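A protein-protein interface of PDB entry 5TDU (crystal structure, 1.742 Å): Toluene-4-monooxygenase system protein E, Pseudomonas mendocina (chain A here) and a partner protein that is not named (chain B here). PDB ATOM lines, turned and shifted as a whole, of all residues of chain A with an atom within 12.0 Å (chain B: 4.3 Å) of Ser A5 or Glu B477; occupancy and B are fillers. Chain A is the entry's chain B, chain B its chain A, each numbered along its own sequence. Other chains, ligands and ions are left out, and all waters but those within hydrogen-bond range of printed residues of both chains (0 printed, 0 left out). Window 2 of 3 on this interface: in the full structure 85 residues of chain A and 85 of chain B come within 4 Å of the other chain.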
ATOM      1  N   SER A   2       2.782 -24.124  -2.835  1.00  0.00           N
ATOM      2  CA  SER A   2       3.041 -22.744  -2.439  1.00  0.00           C
ATOM      3  C   SER A   2       2.608 -22.501  -0.987  1.00  0.00           C
ATOM      4  O   SER A   2       2.113 -23.410  -0.317  1.00  0.00           O
ATOM      5  CB  SER A   2       2.317 -21.779  -3.388  1.00  0.00           C
ATOM      6  OG  SER A   2       2.727 -20.436  -3.183  1.00  0.00           O
ATOM      7  N   PHE A   3       2.811 -21.277  -0.506  1.00  0.00           N
ATOM      8  CA  PHE A   3       2.349 -20.889   0.826  1.00  0.00           C
ATOM      9  C   PHE A   3       0.916 -20.387   0.759  1.00  0.00           C
ATOM     10  O   PHE A   3       0.568 -19.602  -0.122  1.00  0.00           O
ATOM     11  CB  PHE A   3       3.247 -19.805   1.425  1.00  0.00           C
ATOM     12  CG  PHE A   3       4.564 -20.316   1.916  1.00  0.00           C
ATOM     13  CD1 PHE A   3       4.621 -21.366   2.819  1.00  0.00           C
ATOM     14  CD2 PHE A   3       5.748 -19.756   1.467  1.00  0.00           C
ATOM     15  CE1 PHE A   3       5.840 -21.843   3.274  1.00  0.00           C
ATOM     16  CE2 PHE A   3       6.968 -20.227   1.914  1.00  0.00           C
ATOM     17  CZ  PHE A   3       7.013 -21.273   2.820  1.00  0.00           C
ATOM     18  N   GLU A   4       0.080 -20.831   1.689  1.00  0.00           N
ATOM     19  CA  GLU A   4      -1.292 -20.346   1.709  1.00  0.00           C
ATOM     20  C   GLU A   4      -1.522 -19.415   2.888  1.00  0.00           C
ATOM     21  O   GLU A   4      -0.706 -19.334   3.805  1.00  0.00           O
ATOM     22  CB  GLU A   4      -2.284 -21.508   1.741  1.00  0.00           C
ATOM     23  CG  GLU A   4      -2.175 -22.414   2.947  1.00  0.00           C
ATOM     24  CD  GLU A   4      -3.277 -23.457   2.972  1.00  0.00           C
ATOM     25  OE1 GLU A   4      -2.958 -24.657   2.826  1.00  0.00           O
ATOM     26  OE2 GLU A   4      -4.460 -23.074   3.134  1.00  0.00           O
ATOM     27  N   SER A   5      -2.635 -18.696   2.849  1.00  0.00           N
ATOM     28  CA  SER A   5      -2.952 -17.765   3.914  1.00  0.00           C
ATOM     29  C   SER A   5      -3.900 -18.429   4.899  1.00  0.00           C
ATOM     30  O   SER A   5      -4.833 -19.129   4.504  1.00  0.00           O
ATOM     31  CB  SER A   5      -3.565 -16.485   3.343  1.00  0.00           C
ATOM     32  OG  SER A   5      -3.837 -15.543   4.367  1.00  0.00           O
ATOM     33  N   LYS A   6      -3.649 -18.210   6.182  1.00  0.00           N
ATOM     34  CA  LYS A   6      -4.494 -18.757   7.232  1.00  0.00           C
ATOM     35  C   LYS A   6      -4.744 -17.681   8.274  1.00  0.00           C
ATOM     36  O   LYS A   6      -3.937 -16.775   8.439  1.00  0.00           O
ATOM     37  CB  LYS A   6      -3.851 -19.994   7.860  1.00  0.00           C
ATOM     38  CG  LYS A   6      -3.601 -21.109   6.854  1.00  0.00           C
ATOM     39  CD  LYS A   6      -3.028 -22.343   7.508  1.00  0.00           C
ATOM     40  CE  LYS A   6      -2.834 -23.449   6.490  1.00  0.00           C
ATOM     41  NZ  LYS A   6      -2.011 -24.571   7.024  1.00  0.00           N
ATOM     42  N   LYS A   7      -5.875 -17.761   8.956  1.00  0.00           N
ATOM     43  CA  LYS A   7      -6.172 -16.770   9.979  1.00  0.00           C
ATOM     44  C   LYS A   7      -5.609 -17.213  11.323  1.00  0.00           C
ATOM     45  O   LYS A   7      -5.201 -18.362  11.486  1.00  0.00           O
ATOM     46  CB  LYS A   7      -7.676 -16.521  10.078  1.00  0.00           C
ATOM     47  CG  LYS A   7      -8.518 -17.763  10.253  1.00  0.00           C
ATOM     48  CD  LYS A   7      -9.984 -17.459   9.951  1.00  0.00           C
ATOM     49  CE  LYS A   7     -10.900 -18.487  10.596  1.00  0.00           C
ATOM     50  NZ  LYS A   7     -12.328 -18.251  10.266  1.00  0.00           N
ATOM     51  N   PRO A   8      -5.563 -16.285  12.281  1.00  0.00           N
ATOM     52  CA  PRO A   8      -5.142 -16.658  13.635  1.00  0.00           C
ATOM     53  C   PRO A   8      -6.037 -17.742  14.241  1.00  0.00           C
ATOM     54  O   PRO A   8      -7.236 -17.818  13.935  1.00  0.00           O
ATOM     55  CB  PRO A   8      -5.261 -15.343  14.407  1.00  0.00           C
ATOM     56  CG  PRO A   8      -5.041 -14.284  13.368  1.00  0.00           C
ATOM     57  CD  PRO A   8      -5.707 -14.827  12.124  1.00  0.00           C
ATOM     58  N   MET A   9      -5.453 -18.574  15.098  1.00  0.00           N
ATOM     59  CA  MET A   9      -6.175 -19.672  15.715  1.00  0.00           C
ATOM     60  C   MET A   9      -6.431 -19.306  17.173  1.00  0.00           C
ATOM     61  O   MET A   9      -5.683 -18.523  17.755  1.00  0.00           O
ATOM     62  CB  MET A   9      -5.389 -20.979  15.589  1.00  0.00           C
ATOM     63  CG  MET A   9      -5.104 -21.420  14.145  1.00  0.00           C
ATOM     64  SD  MET A   9      -3.846 -22.719  14.026  1.00  0.00           S
ATOM     65  CE  MET A   9      -2.368 -21.783  14.413  1.00  0.00           C
ATOM     66  N   SER A  13      -1.802 -24.495  17.452  1.00  0.00           N
ATOM     67  CA  SER A  13      -2.174 -25.228  16.247  1.00  0.00           C
ATOM     68  C   SER A  13      -2.523 -26.697  16.552  1.00  0.00           C
ATOM     69  O   SER A  13      -3.425 -27.261  15.930  1.00  0.00           O
ATOM     70  CB  SER A  13      -1.055 -25.141  15.200  1.00  0.00           C
ATOM     71  OG  SER A  13       0.216 -25.418  15.777  1.00  0.00           O
ATOM     72  N   GLN B 154       2.128 -15.853  14.670  1.00  0.00           N
ATOM     73  CA  GLN B 154       3.517 -15.982  15.086  1.00  0.00           C
ATOM     74  C   GLN B 154       3.628 -16.341  16.572  1.00  0.00           C
ATOM     75  O   GLN B 154       4.625 -16.923  16.992  1.00  0.00           O
ATOM     76  CB  GLN B 154       4.293 -14.702  14.789  1.00  0.00           C
ATOM     77  CG  GLN B 154       4.701 -14.598  13.315  1.00  0.00           C
ATOM     78  CD  GLN B 154       5.510 -13.359  13.001  1.00  0.00           C
ATOM     79  OE1 GLN B 154       5.490 -12.385  13.745  1.00  0.00           O
ATOM     80  NE2 GLN B 154       6.233 -13.391  11.885  1.00  0.00           N
ATOM     81  N   SER B 475       1.967 -20.886   7.151  1.00  0.00           N
ATOM     82  CA  SER B 475       1.259 -19.879   6.357  1.00  0.00           C
ATOM     83  C   SER B 475       2.164 -18.688   6.085  1.00  0.00           C
ATOM     84  O   SER B 475       3.190 -18.526   6.736  1.00  0.00           O
ATOM     85  CB  SER B 475      -0.035 -19.430   7.057  1.00  0.00           C
ATOM     86  OG  SER B 475       0.216 -18.614   8.193  1.00  0.00           O
ATOM     87  N   ILE B 476       1.785 -17.854   5.122  1.00  0.00           N
ATOM     88  CA  ILE B 476       2.621 -16.718   4.740  1.00  0.00           C
ATOM     89  C   ILE B 476       2.754 -15.751   5.912  1.00  0.00           C
ATOM     90  O   ILE B 476       3.804 -15.131   6.098  1.00  0.00           O
ATOM     91  CB  ILE B 476       2.071 -16.000   3.486  1.00  0.00           C
ATOM     92  CG1 ILE B 476       3.092 -14.992   2.950  1.00  0.00           C
ATOM     93  CG2 ILE B 476       0.757 -15.315   3.786  1.00  0.00           C
ATOM     94  CD1 ILE B 476       4.316 -15.631   2.300  1.00  0.00           C
ATOM     95  N   GLU B 477       1.688 -15.637   6.704  1.00  0.00           N
ATOM     96  CA  GLU B 477       1.667 -14.718   7.839  1.00  0.00           C
ATOM     97  C   GLU B 477       2.761 -14.998   8.860  1.00  0.00           C
ATOM     98  O   GLU B 477       3.223 -14.083   9.549  1.00  0.00           O
ATOM     99  CB  GLU B 477       0.307 -14.769   8.535  1.00  0.00           C
ATOM    100  CG  GLU B 477      -0.842 -14.216   7.694  1.00  0.00           C
ATOM    101  CD  GLU B 477      -1.548 -15.279   6.862  1.00  0.00           C
ATOM    102  OE1 GLU B 477      -1.248 -16.479   7.030  1.00  0.00           O
ATOM    103  OE2 GLU B 477      -2.423 -14.914   6.042  1.00  0.00           O
ATOM    104  N   GLU B 478       3.168 -16.259   8.957  1.00  0.00           N
ATOM    105  CA  GLU B 478       4.065 -16.689  10.024  1.00  0.00           C
ATOM    106  C   GLU B 478       5.506 -16.244   9.778  1.00  0.00           C
ATOM    107  O   GLU B 478       6.277 -16.079  10.722  1.00  0.00           O
ATOM    108  CB  GLU B 478       3.986 -18.212  10.192  1.00  0.00           C
ATOM    109  CG  GLU B 478       2.626 -18.698  10.689  1.00  0.00           C
ATOM    110  CD  GLU B 478       2.503 -20.211  10.736  1.00  0.00           C
ATOM    111  OE1 GLU B 478       3.507 -20.908  10.494  1.00  0.00           O
ATOM    112  OE2 GLU B 478       1.389 -20.705  11.011  1.00  0.00           O
ATOM    113  N   MET B 479       5.870 -16.026   8.516  1.00  0.00           N
ATOM    114  CA  MET B 479       7.257 -15.682   8.192  1.00  0.00           C
ATOM    115  C   MET B 479       7.588 -14.235   8.522  1.00  0.00           C
ATOM    116  O   MET B 479       6.747 -13.345   8.387  1.00  0.00           O
ATOM    117  CB  MET B 479       7.543 -15.956   6.726  1.00  0.00           C
ATOM    118  CG  MET B 479       7.376 -17.400   6.371  1.00  0.00           C
ATOM    119  SD  MET B 479       7.893 -17.654   4.682  1.00  0.00           S
ATOM    120  CE  MET B 479       7.240 -16.157   3.923  1.00  0.00           C
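OG of Ser B475 is in hydrogen-bond range of OE1 of Glu B477 (2.8 Å).
Among the printed residues, pairs that only touch across the chains: Phe A3 with Met B479, Glu A4 with Ser B475 and Lys A6 with Ser B475.
N of Ile B476 is in hydrogen-bond range of O of Glu A4 (3.2 Å).
The backbone NH (N) of Lys A6 lies within hydrogen-bond range of the side-chain carboxylate (OE1) of Glu B477 (3.1 Å).
The side-chain carboxylate (OE2) of Glu B477 sits close to the side-chain hydroxyl (OG) of Ser A5.
Glu B477 touches just these residues of chain A: Ser A5 and Lys A6.
Ser B475 touches just these residues of chain A: Glu A4 and Lys A6.
Of chain A, only Glu A4 (3.2 Å) comes within 4 Å of Ile B476.
No residue of chain A comes within 4 Å of Glu B478.
Of the printed residues of chain B, Glu A4 touches Ser B475 (3.3 Å) and Ile B476 (3.2 Å).
Of the printed residues of chain B, Lys A6 touches Ser B475 and Glu B477.
Of the printed residues of chain B, Phe A3 touches Met B479 (3.9 Å).
Ser A2 touches none of the printed residues of chain B.
Met A9 touches none of the printed residues of chain B.
The nearest printed residue of chain B that does not touch Glu A4 is Glu B477 (4.3 Å).
Hydrophobic or aromatic side chains of chain B that line the printed part of chain A: Met B479.
Hydrophobic or aromatic side chains of chain A within 4 Å of the printed part of chain B: Phe A3.
Among the printed residues, 6 pairs touch across the chains.
Among the printed residues, no Asp or Glu carboxylate lies within 4 Å of a Lys or Arg side-chain nitrogen of the other chain.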
